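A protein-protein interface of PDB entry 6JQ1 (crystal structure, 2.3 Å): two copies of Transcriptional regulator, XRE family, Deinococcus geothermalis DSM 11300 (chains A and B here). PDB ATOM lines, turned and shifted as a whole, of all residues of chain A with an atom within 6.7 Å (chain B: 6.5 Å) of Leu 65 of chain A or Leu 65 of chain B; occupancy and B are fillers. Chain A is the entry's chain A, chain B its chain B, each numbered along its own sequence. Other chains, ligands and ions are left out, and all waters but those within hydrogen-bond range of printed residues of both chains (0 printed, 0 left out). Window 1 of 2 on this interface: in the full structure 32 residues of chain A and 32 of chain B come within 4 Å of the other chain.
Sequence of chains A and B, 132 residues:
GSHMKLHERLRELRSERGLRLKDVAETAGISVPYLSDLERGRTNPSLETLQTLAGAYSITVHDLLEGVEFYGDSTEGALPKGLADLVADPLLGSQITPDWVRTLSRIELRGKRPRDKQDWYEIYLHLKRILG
A ring nitrogen (NE2) of His 62 of chain A sits at hydrogen-bond distance from a ring nitrogen (NE2) of His 62 of chain B, 3.0 Å away.
Leu 47 of chain B touches Leu 6 of chain A (CD2 to CD2, 3.5 Å).
Leu 6 of chain B touches Leu 47 of chain A.
CD1 of Leu 47 of chain A touches CD1 of Leu 50 of chain B, at 3.95 Å.
Val 61 of chain A touches Phe 70 of chain B (CG1 to CE2, 3.8 Å).
CD2 of His 62 of chain A touches C of Leu 65 of chain B (3.9 Å).
Glu 66 of chain B touches His 62 of chain A.
CB of His 62 of chain B touches O of Leu 65 of chain A (3.8 Å).
Leu 65 of chain A touches Leu 65 of chain B (CD1 to CD1, 3.6 Å).
Glu 66 of chain A touches His 62 of chain B.
CE2 of Phe 70 of chain A touches CD2 of Leu 47 of chain B (3.7 Å).
Leu 47 of chain A touches Leu 50 of chain B, but with the chains exchanged Leu 50 of chain A does not touch Leu 47 of chain B (4.2 Å).
Val 61 of chain A touches Phe 70 of chain B, but with the chains exchanged Phe 70 of chain A does not touch Val 61 of chain B (4.1 Å).
His 62 of chain A touches Leu 65 of chain B, and with the chains exchanged Leu 65 of chain A touches His 62 of chain B.
His 62 of chain A touches Glu 66 of chain B, and with the chains exchanged Glu 66 of chain A touches His 62 of chain B.
Positions printed for both chains: 6, 9, 47, 50, 59, 60, 61, 62, 63, 64, 65, 66, 67, 68, 69 and 70.
Leu 65 of chain A touches just these residues of chain B: His 62 (3.8 Å) and Leu 65 (3.6 Å).
Of the printed residues of chain B, Glu 66 of chain A touches His 62 (3.7 Å).
Leu 65 of chain B touches just these residues of chain A: His 62 and Leu 65.
Of the printed residues of chain A, Phe 70 of chain B touches Val 61 (3.8 Å).
The nearest residue of chain B that does not touch Leu 65 of chain A is Val 61 of chain B (4.1 Å).
The nearest printed residue of chain A that does not touch Leu 6 of chain B is Val 61 of chain A (8.2 Å).
Along chain A the printed residues that touch a printed residue of chain B span positions 6 to 70.
O of Glu 66 of chain B lies within hydrogen-bond range of NE of Arg 9 of chain B (3.4 Å).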
ATOM      1  N   LEU A   6     -23.228  -1.517 -13.043  1.00  0.00           N
ATOM      2  CA  LEU A   6     -24.689  -1.417 -12.983  1.00  0.00           C
ATOM      3  C   LEU A   6     -25.354  -2.763 -13.269  1.00  0.00           C
ATOM      4  O   LEU A   6     -26.220  -3.213 -12.508  1.00  0.00           O
ATOM      5  CB  LEU A   6     -25.184  -0.339 -13.946  1.00  0.00           C
ATOM      6  CG  LEU A   6     -26.699  -0.379 -14.192  1.00  0.00           C
ATOM      7  CD1 LEU A   6     -27.501  -0.043 -12.930  1.00  0.00           C
ATOM      8  CD2 LEU A   6     -27.145   0.482 -15.384  1.00  0.00           C
ATOM      9  N   ARG A   9     -25.011  -5.052 -10.477  1.00  0.00           N
ATOM     10  CA  ARG A   9     -25.934  -4.720  -9.396  1.00  0.00           C
ATOM     11  C   ARG A   9     -27.334  -5.250  -9.685  1.00  0.00           C
ATOM     12  O   ARG A   9     -28.003  -5.779  -8.788  1.00  0.00           O
ATOM     13  CB  ARG A   9     -25.959  -3.204  -9.202  1.00  0.00           C
ATOM     14  CG  ARG A   9     -27.025  -2.700  -8.245  1.00  0.00           C
ATOM     15  CD  ARG A   9     -26.757  -3.129  -6.807  1.00  0.00           C
ATOM     16  NE  ARG A   9     -27.508  -2.306  -5.863  1.00  0.00           N
ATOM     17  CZ  ARG A   9     -27.855  -2.685  -4.636  1.00  0.00           C
ATOM     18  NH1 ARG A   9     -27.531  -3.889  -4.187  1.00  0.00           N
ATOM     19  NH2 ARG A   9     -28.540  -1.856  -3.859  1.00  0.00           N
ATOM     20  N   LEU A  47     -33.565   5.801 -17.704  1.00  0.00           N
ATOM     21  CA  LEU A  47     -34.007   6.190 -16.369  1.00  0.00           C
ATOM     22  C   LEU A  47     -35.413   5.674 -16.083  1.00  0.00           C
ATOM     23  O   LEU A  47     -35.686   5.174 -14.984  1.00  0.00           O
ATOM     24  CB  LEU A  47     -33.941   7.709 -16.213  1.00  0.00           C
ATOM     25  CG  LEU A  47     -32.522   8.247 -16.032  1.00  0.00           C
ATOM     26  CD1 LEU A  47     -32.512   9.757 -15.917  1.00  0.00           C
ATOM     27  CD2 LEU A  47     -31.875   7.607 -14.816  1.00  0.00           C
ATOM     28  N   LEU A  50     -35.071   2.111 -15.395  1.00  0.00           N
ATOM     29  CA  LEU A  50     -34.374   1.920 -14.127  1.00  0.00           C
ATOM     30  C   LEU A  50     -35.321   2.082 -12.945  1.00  0.00           C
ATOM     31  O   LEU A  50     -35.252   1.317 -11.975  1.00  0.00           O
ATOM     32  CB  LEU A  50     -33.218   2.915 -14.030  1.00  0.00           C
ATOM     33  CG  LEU A  50     -31.982   2.463 -13.259  1.00  0.00           C
ATOM     34  CD1 LEU A  50     -31.677   1.001 -13.553  1.00  0.00           C
ATOM     35  CD2 LEU A  50     -30.793   3.347 -13.621  1.00  0.00           C
ATOM     36  N   ILE A  59     -37.307  -0.698  -3.871  1.00  0.00           N
ATOM     37  CA  ILE A  59     -36.291   0.237  -3.416  1.00  0.00           C
ATOM     38  C   ILE A  59     -36.331   1.466  -4.313  1.00  0.00           C
ATOM     39  O   ILE A  59     -36.952   1.469  -5.379  1.00  0.00           O
ATOM     40  CB  ILE A  59     -34.874  -0.380  -3.397  1.00  0.00           C
ATOM     41  CG1 ILE A  59     -34.483  -0.836  -4.806  1.00  0.00           C
ATOM     42  CG2 ILE A  59     -34.783  -1.522  -2.373  1.00  0.00           C
ATOM     43  CD1 ILE A  59     -33.073  -1.375  -4.915  1.00  0.00           C
ATOM     44  N   THR A  60     -35.670   2.526  -3.855  1.00  0.00           N
ATOM     45  CA  THR A  60     -35.529   3.750  -4.628  1.00  0.00           C
ATOM     46  C   THR A  60     -34.470   3.557  -5.713  1.00  0.00           C
ATOM     47  O   THR A  60     -33.602   2.684  -5.617  1.00  0.00           O
ATOM     48  CB  THR A  60     -35.124   4.903  -3.700  1.00  0.00           C
ATOM     49  OG1 THR A  60     -35.826   4.788  -2.454  1.00  0.00           O
ATOM     50  CG2 THR A  60     -35.449   6.257  -4.322  1.00  0.00           C
ATOM     51  N   VAL A  61     -34.564   4.372  -6.772  1.00  0.00           N
ATOM     52  CA  VAL A  61     -33.511   4.400  -7.788  1.00  0.00           C
ATOM     53  C   VAL A  61     -32.175   4.766  -7.153  1.00  0.00           C
ATOM     54  O   VAL A  61     -31.129   4.191  -7.487  1.00  0.00           O
ATOM     55  CB  VAL A  61     -33.880   5.374  -8.927  1.00  0.00           C
ATOM     56  CG1 VAL A  61     -32.714   5.535  -9.893  1.00  0.00           C
ATOM     57  CG2 VAL A  61     -35.113   4.906  -9.665  1.00  0.00           C
ATOM     58  N   HIS A  62     -32.194   5.733  -6.228  1.00  0.00           N
ATOM     59  CA  HIS A  62     -30.981   6.138  -5.522  1.00  0.00           C
ATOM     60  C   HIS A  62     -30.365   4.967  -4.764  1.00  0.00           C
ATOM     61  O   HIS A  62     -29.148   4.750  -4.826  1.00  0.00           O
ATOM     62  CB  HIS A  62     -31.314   7.298  -4.575  1.00  0.00           C
ATOM     63  CG  HIS A  62     -30.154   7.774  -3.757  1.00  0.00           C
ATOM     64  ND1 HIS A  62     -30.087   7.603  -2.390  1.00  0.00           N
ATOM     65  CD2 HIS A  62     -29.020   8.423  -4.110  1.00  0.00           C
ATOM     66  CE1 HIS A  62     -28.959   8.121  -1.937  1.00  0.00           C
ATOM     67  NE2 HIS A  62     -28.294   8.627  -2.962  1.00  0.00           N
ATOM     68  N   ASP A  63     -31.193   4.190  -4.055  1.00  0.00           N
ATOM     69  CA  ASP A  63     -30.698   3.025  -3.324  1.00  0.00           C
ATOM     70  C   ASP A  63     -30.220   1.932  -4.274  1.00  0.00           C
ATOM     71  O   ASP A  63     -29.241   1.232  -3.983  1.00  0.00           O
ATOM     72  CB  ASP A  63     -31.780   2.495  -2.381  1.00  0.00           C
ATOM     73  CG  ASP A  63     -32.012   3.404  -1.185  1.00  0.00           C
ATOM     74  OD1 ASP A  63     -31.057   4.102  -0.783  1.00  0.00           O
ATOM     75  OD2 ASP A  63     -33.143   3.417  -0.650  1.00  0.00           O
ATOM     76  N   LEU A  64     -30.905   1.760  -5.411  1.00  0.00           N
ATOM     77  CA  LEU A  64     -30.471   0.771  -6.394  1.00  0.00           C
ATOM     78  C   LEU A  64     -29.071   1.085  -6.897  1.00  0.00           C
ATOM     79  O   LEU A  64     -28.247   0.179  -7.072  1.00  0.00           O
ATOM     80  CB  LEU A  64     -31.469   0.728  -7.556  1.00  0.00           C
ATOM     81  CG  LEU A  64     -31.242  -0.221  -8.738  1.00  0.00           C
ATOM     82  CD1 LEU A  64     -32.579  -0.565  -9.379  1.00  0.00           C
ATOM     83  CD2 LEU A  64     -30.307   0.377  -9.787  1.00  0.00           C
ATOM     84  N   LEU A  65     -28.784   2.363  -7.136  1.00  0.00           N
ATOM     85  CA  LEU A  65     -27.483   2.774  -7.646  1.00  0.00           C
ATOM     86  C   LEU A  65     -26.419   2.884  -6.562  1.00  0.00           C
ATOM     87  O   LEU A  65     -25.273   3.217  -6.882  1.00  0.00           O
ATOM     88  CB  LEU A  65     -27.600   4.093  -8.414  1.00  0.00           C
ATOM     89  CG  LEU A  65     -28.191   3.982  -9.822  1.00  0.00           C
ATOM     90  CD1 LEU A  65     -28.110   5.316 -10.539  1.00  0.00           C
ATOM     91  CD2 LEU A  65     -27.490   2.896 -10.625  1.00  0.00           C
ATOM     92  N   GLU A  66     -26.758   2.619  -5.303  1.00  0.00           N
ATOM     93  CA  GLU A  66     -25.757   2.661  -4.246  1.00  0.00           C
ATOM     94  C   GLU A  66     -24.716   1.574  -4.475  1.00  0.00           C
ATOM     95  O   GLU A  66     -25.056   0.409  -4.701  1.00  0.00           O
ATOM     96  CB  GLU A  66     -26.422   2.470  -2.885  1.00  0.00           C
ATOM     97  CG  GLU A  66     -25.433   2.274  -1.749  1.00  0.00           C
ATOM     98  CD  GLU A  66     -26.087   2.357  -0.388  1.00  0.00           C
ATOM     99  OE1 GLU A  66     -25.693   1.584   0.511  1.00  0.00           O
ATOM    100  OE2 GLU A  66     -26.998   3.194  -0.218  1.00  0.00           O
ATOM    101  N   GLY A  67     -23.442   1.960  -4.427  1.00  0.00           N
ATOM    102  CA  GLY A  67     -22.360   1.032  -4.684  1.00  0.00           C
ATOM    103  C   GLY A  67     -22.144   0.673  -6.136  1.00  0.00           C
ATOM    104  O   GLY A  67     -21.450  -0.309  -6.418  1.00  0.00           O
ATOM    105  N   VAL A  68     -22.709   1.435  -7.066  1.00  0.00           N
ATOM    106  CA  VAL A  68     -22.566   1.188  -8.498  1.00  0.00           C
ATOM    107  C   VAL A  68     -21.537   2.164  -9.057  1.00  0.00           C
ATOM    108  O   VAL A  68     -21.619   3.371  -8.799  1.00  0.00           O
ATOM    109  CB  VAL A  68     -23.921   1.349  -9.214  1.00  0.00           C
ATOM    110  CG1 VAL A  68     -23.741   1.418 -10.724  1.00  0.00           C
ATOM    111  CG2 VAL A  68     -24.871   0.219  -8.831  1.00  0.00           C
ATOM    112  N   GLU A  69     -20.684   1.634  -9.932  1.00  0.00           N
ATOM    113  CA  GLU A  69     -19.575   2.377 -10.575  1.00  0.00           C
ATOM    114  C   GLU A  69     -19.834   2.490 -12.082  1.00  0.00           C
ATOM    115  O   GLU A  69     -20.131   1.457 -12.694  1.00  0.00           O
ATOM    116  CB  GLU A  69     -18.324   1.532 -10.341  1.00  0.00           C
ATOM    117  CG  GLU A  69     -17.008   2.251 -10.533  1.00  0.00           C
ATOM    118  CD  GLU A  69     -15.819   1.350 -10.247  1.00  0.00           C
ATOM    119  OE1 GLU A  69     -16.038   0.235  -9.743  1.00  0.00           O
ATOM    120  OE2 GLU A  69     -14.683   1.762 -10.535  1.00  0.00           O
ATOM    121  N   PHE A  70     -19.750   3.700 -12.645  1.00  0.00           N
ATOM    122  CA  PHE A  70     -19.878   3.906 -14.080  1.00  0.00           C
ATOM    123  C   PHE A  70     -18.494   4.171 -14.658  1.00  0.00           C
ATOM    124  O   PHE A  70     -17.777   5.057 -14.179  1.00  0.00           O
ATOM    125  CB  PHE A  70     -20.826   5.074 -14.353  1.00  0.00           C
ATOM    126  CG  PHE A  70     -22.247   4.791 -13.960  1.00  0.00           C
ATOM    127  CD1 PHE A  70     -22.673   4.986 -12.656  1.00  0.00           C
ATOM    128  CD2 PHE A  70     -23.152   4.298 -14.889  1.00  0.00           C
ATOM    129  CE1 PHE A  70     -23.976   4.706 -12.289  1.00  0.00           C
ATOM    130  CE2 PHE A  70     -24.459   4.016 -14.526  1.00  0.00           C
ATOM    131  CZ  PHE A  70     -24.871   4.220 -13.226  1.00  0.00           C
ATOM    132  N   LEU B   6     -35.808  15.538 -11.120  1.00  0.00           N
ATOM    133  CA  LEU B   6     -34.456  15.408 -11.662  1.00  0.00           C
ATOM    134  C   LEU B   6     -33.996  16.687 -12.352  1.00  0.00           C
ATOM    135  O   LEU B   6     -32.858  17.131 -12.154  1.00  0.00           O
ATOM    136  CB  LEU B   6     -34.374  14.215 -12.616  1.00  0.00           C
ATOM    137  CG  LEU B   6     -33.028  13.982 -13.309  1.00  0.00           C
ATOM    138  CD1 LEU B   6     -31.855  14.080 -12.333  1.00  0.00           C
ATOM    139  CD2 LEU B   6     -33.025  12.637 -14.015  1.00  0.00           C
ATOM    140  N   ARG B   9     -33.163  19.281  -9.745  1.00  0.00           N
ATOM    141  CA  ARG B   9     -31.870  19.022  -9.121  1.00  0.00           C
ATOM    142  C   ARG B   9     -30.726  19.498 -10.006  1.00  0.00           C
ATOM    143  O   ARG B   9     -29.722  20.023  -9.506  1.00  0.00           O
ATOM    144  CB  ARG B   9     -31.729  17.525  -8.846  1.00  0.00           C
ATOM    145  CG  ARG B   9     -30.349  17.096  -8.364  1.00  0.00           C
ATOM    146  CD  ARG B   9     -30.211  17.172  -6.846  1.00  0.00           C
ATOM    147  NE  ARG B   9     -29.051  16.413  -6.387  1.00  0.00           N
ATOM    148  CZ  ARG B   9     -28.030  16.927  -5.706  1.00  0.00           C
ATOM    149  NH1 ARG B   9     -28.027  18.210  -5.383  1.00  0.00           N
ATOM    150  NH2 ARG B   9     -27.016  16.152  -5.338  1.00  0.00           N
ATOM    151  N   LEU B  47     -28.535   7.690 -19.240  1.00  0.00           N
ATOM    152  CA  LEU B  47     -27.614   7.343 -18.164  1.00  0.00           C
ATOM    153  C   LEU B  47     -26.209   7.843 -18.475  1.00  0.00           C
ATOM    154  O   LEU B  47     -25.510   8.358 -17.595  1.00  0.00           O
ATOM    155  CB  LEU B  47     -27.605   5.828 -17.971  1.00  0.00           C
ATOM    156  CG  LEU B  47     -27.313   5.309 -16.565  1.00  0.00           C
ATOM    157  CD1 LEU B  47     -28.145   6.059 -15.535  1.00  0.00           C
ATOM    158  CD2 LEU B  47     -27.596   3.819 -16.501  1.00  0.00           C
ATOM    159  N   LEU B  50     -25.973  11.423 -17.742  1.00  0.00           N
ATOM    160  CA  LEU B  50     -25.878  11.680 -16.308  1.00  0.00           C
ATOM    161  C   LEU B  50     -24.446  11.544 -15.811  1.00  0.00           C
ATOM    162  O   LEU B  50     -24.004  12.322 -14.957  1.00  0.00           O
ATOM    163  CB  LEU B  50     -26.806  10.741 -15.537  1.00  0.00           C
ATOM    164  CG  LEU B  50     -28.211  11.270 -15.252  1.00  0.00           C
ATOM    165  CD1 LEU B  50     -28.948  10.335 -14.306  1.00  0.00           C
ATOM    166  CD2 LEU B  50     -28.141  12.678 -14.682  1.00  0.00           C
ATOM    167  N   ILE B  59     -19.214  14.980  -8.831  1.00  0.00           N
ATOM    168  CA  ILE B  59     -19.954  14.088  -7.948  1.00  0.00           C
ATOM    169  C   ILE B  59     -20.282  12.807  -8.701  1.00  0.00           C
ATOM    170  O   ILE B  59     -20.203  12.743  -9.930  1.00  0.00           O
ATOM    171  CB  ILE B  59     -21.243  14.731  -7.381  1.00  0.00           C
ATOM    172  CG1 ILE B  59     -22.210  15.084  -8.515  1.00  0.00           C
ATOM    173  CG2 ILE B  59     -20.908  15.953  -6.522  1.00  0.00           C
ATOM    174  CD1 ILE B  59     -23.501  15.720  -8.042  1.00  0.00           C
ATOM    175  N   THR B  60     -20.645  11.775  -7.945  1.00  0.00           N
ATOM    176  CA  THR B  60     -21.061  10.518  -8.548  1.00  0.00           C
ATOM    177  C   THR B  60     -22.526  10.603  -8.965  1.00  0.00           C
ATOM    178  O   THR B  60     -23.292  11.421  -8.447  1.00  0.00           O
ATOM    179  CB  THR B  60     -20.889   9.378  -7.543  1.00  0.00           C
ATOM    180  OG1 THR B  60     -21.783   9.579  -6.444  1.00  0.00           O
ATOM    181  CG2 THR B  60     -19.458   9.338  -7.017  1.00  0.00           C
ATOM    182  N   VAL B  61     -22.910   9.755  -9.927  1.00  0.00           N
ATOM    183  CA  VAL B  61     -24.309   9.694 -10.352  1.00  0.00           C
ATOM    184  C   VAL B  61     -25.208   9.383  -9.162  1.00  0.00           C
ATOM    185  O   VAL B  61     -26.278   9.985  -8.992  1.00  0.00           O
ATOM    186  CB  VAL B  61     -24.490   8.665 -11.483  1.00  0.00           C
ATOM    187  CG1 VAL B  61     -25.975   8.513 -11.845  1.00  0.00           C
ATOM    188  CG2 VAL B  61     -23.662   9.052 -12.707  1.00  0.00           C
ATOM    189  N   HIS B  62     -24.777   8.444  -8.314  1.00  0.00           N
ATOM    190  CA  HIS B  62     -25.526   8.108  -7.107  1.00  0.00           C
ATOM    191  C   HIS B  62     -25.708   9.328  -6.207  1.00  0.00           C
ATOM    192  O   HIS B  62     -26.814   9.586  -5.716  1.00  0.00           O
ATOM    193  CB  HIS B  62     -24.827   6.962  -6.369  1.00  0.00           C
ATOM    194  CG  HIS B  62     -25.321   6.748  -4.974  1.00  0.00           C
ATOM    195  ND1 HIS B  62     -24.570   7.065  -3.864  1.00  0.00           N
ATOM    196  CD2 HIS B  62     -26.493   6.257  -4.507  1.00  0.00           C
ATOM    197  CE1 HIS B  62     -25.257   6.776  -2.773  1.00  0.00           C
ATOM    198  NE2 HIS B  62     -26.427   6.284  -3.136  1.00  0.00           N
ATOM    199  N   ASP B  63     -24.637  10.102  -5.992  1.00  0.00           N
ATOM    200  CA  ASP B  63     -24.753  11.341  -5.223  1.00  0.00           C
ATOM    201  C   ASP B  63     -25.575  12.401  -5.955  1.00  0.00           C
ATOM    202  O   ASP B  63     -26.298  13.171  -5.314  1.00  0.00           O
ATOM    203  CB  ASP B  63     -23.363  11.877  -4.854  1.00  0.00           C
ATOM    204  CG  ASP B  63     -22.764  11.173  -3.647  1.00  0.00           C
ATOM    205  OD1 ASP B  63     -23.500  10.402  -2.994  1.00  0.00           O
ATOM    206  OD2 ASP B  63     -21.565  11.382  -3.349  1.00  0.00           O
ATOM    207  N   LEU B  64     -25.477  12.459  -7.288  1.00  0.00           N
ATOM    208  CA  LEU B  64     -26.309  13.387  -8.053  1.00  0.00           C
ATOM    209  C   LEU B  64     -27.788  13.069  -7.884  1.00  0.00           C
ATOM    210  O   LEU B  64     -28.610  13.977  -7.718  1.00  0.00           O
ATOM    211  CB  LEU B  64     -25.920  13.341  -9.537  1.00  0.00           C
ATOM    212  CG  LEU B  64     -26.720  14.159 -10.564  1.00  0.00           C
ATOM    213  CD1 LEU B  64     -25.842  14.500 -11.764  1.00  0.00           C
ATOM    214  CD2 LEU B  64     -27.987  13.443 -11.041  1.00  0.00           C
ATOM    215  N   LEU B  65     -28.150  11.787  -7.956  1.00  0.00           N
ATOM    216  CA  LEU B  65     -29.544  11.390  -7.820  1.00  0.00           C
ATOM    217  C   LEU B  65     -30.051  11.461  -6.385  1.00  0.00           C
ATOM    218  O   LEU B  65     -31.250  11.268  -6.165  1.00  0.00           O
ATOM    219  CB  LEU B  65     -29.753   9.982  -8.377  1.00  0.00           C
ATOM    220  CG  LEU B  65     -29.650   9.836  -9.895  1.00  0.00           C
ATOM    221  CD1 LEU B  65     -29.888   8.395 -10.286  1.00  0.00           C
ATOM    222  CD2 LEU B  65     -30.648  10.746 -10.594  1.00  0.00           C
ATOM    223  N   GLU B  66     -29.181  11.728  -5.413  1.00  0.00           N
ATOM    224  CA  GLU B  66     -29.627  11.847  -4.031  1.00  0.00           C
ATOM    225  C   GLU B  66     -30.648  12.969  -3.906  1.00  0.00           C
ATOM    226  O   GLU B  66     -30.420  14.088  -4.373  1.00  0.00           O
ATOM    227  CB  GLU B  66     -28.436  12.133  -3.118  1.00  0.00           C
ATOM    228  CG  GLU B  66     -28.815  12.256  -1.653  1.00  0.00           C
ATOM    229  CD  GLU B  66     -27.850  13.119  -0.868  1.00  0.00           C
ATOM    230  OE1 GLU B  66     -26.932  13.698  -1.486  1.00  0.00           O
ATOM    231  OE2 GLU B  66     -28.014  13.221   0.366  1.00  0.00           O
ATOM    232  N   GLY B  67     -31.777  12.664  -3.273  1.00  0.00           N
ATOM    233  CA  GLY B  67     -32.844  13.628  -3.114  1.00  0.00           C
ATOM    234  C   GLY B  67     -33.732  13.803  -4.324  1.00  0.00           C
ATOM    235  O   GLY B  67     -34.582  14.703  -4.324  1.00  0.00           O
ATOM    236  N   VAL B  68     -33.571  12.975  -5.351  1.00  0.00           N
ATOM    237  CA  VAL B  68     -34.353  13.082  -6.576  1.00  0.00           C
ATOM    238  C   VAL B  68     -35.494  12.075  -6.526  1.00  0.00           C
ATOM    239  O   VAL B  68     -35.268  10.878  -6.298  1.00  0.00           O
ATOM    240  CB  VAL B  68     -33.473  12.862  -7.819  1.00  0.00           C
ATOM    241  CG1 VAL B  68     -34.330  12.821  -9.067  1.00  0.00           C
ATOM    242  CG2 VAL B  68     -32.427  13.959  -7.925  1.00  0.00           C
ATOM    243  N   GLU B  69     -36.714  12.562  -6.737  1.00  0.00           N
ATOM    244  CA  GLU B  69     -37.912  11.739  -6.820  1.00  0.00           C
ATOM    245  C   GLU B  69     -38.317  11.646  -8.285  1.00  0.00           C
ATOM    246  O   GLU B  69     -38.406  12.669  -8.969  1.00  0.00           O
ATOM    247  CB  GLU B  69     -39.037  12.381  -6.009  1.00  0.00           C
ATOM    248  CG  GLU B  69     -40.006  11.409  -5.365  1.00  0.00           C
ATOM    249  CD  GLU B  69     -40.965  12.109  -4.423  1.00  0.00           C
ATOM    250  OE1 GLU B  69     -41.039  13.355  -4.478  1.00  0.00           O
ATOM    251  OE2 GLU B  69     -41.636  11.419  -3.627  1.00  0.00           O
ATOM    252  N   PHE B  70     -38.561  10.424  -8.764  1.00  0.00           N
ATOM    253  CA  PHE B  70     -38.728  10.183 -10.193  1.00  0.00           C
ATOM    254  C   PHE B  70     -40.172  10.227 -10.680  1.00  0.00           C
ATOM    255  O   PHE B  70     -40.391  10.178 -11.896  1.00  0.00           O
ATOM    256  CB  PHE B  70     -38.047   8.872 -10.609  1.00  0.00           C
ATOM    257  CG  PHE B  70     -36.592   9.031 -10.944  1.00  0.00           C
ATOM    258  CD1 PHE B  70     -36.200   9.434 -12.211  1.00  0.00           C
ATOM    259  CD2 PHE B  70     -35.616   8.800  -9.988  1.00  0.00           C
ATOM    260  CE1 PHE B  70     -34.863   9.593 -12.524  1.00  0.00           C
ATOM    261  CE2 PHE B  70     -34.276   8.957 -10.293  1.00  0.00           C
ATOM    262  CZ  PHE B  70     -33.899   9.354 -11.564  1.00  0.00           C
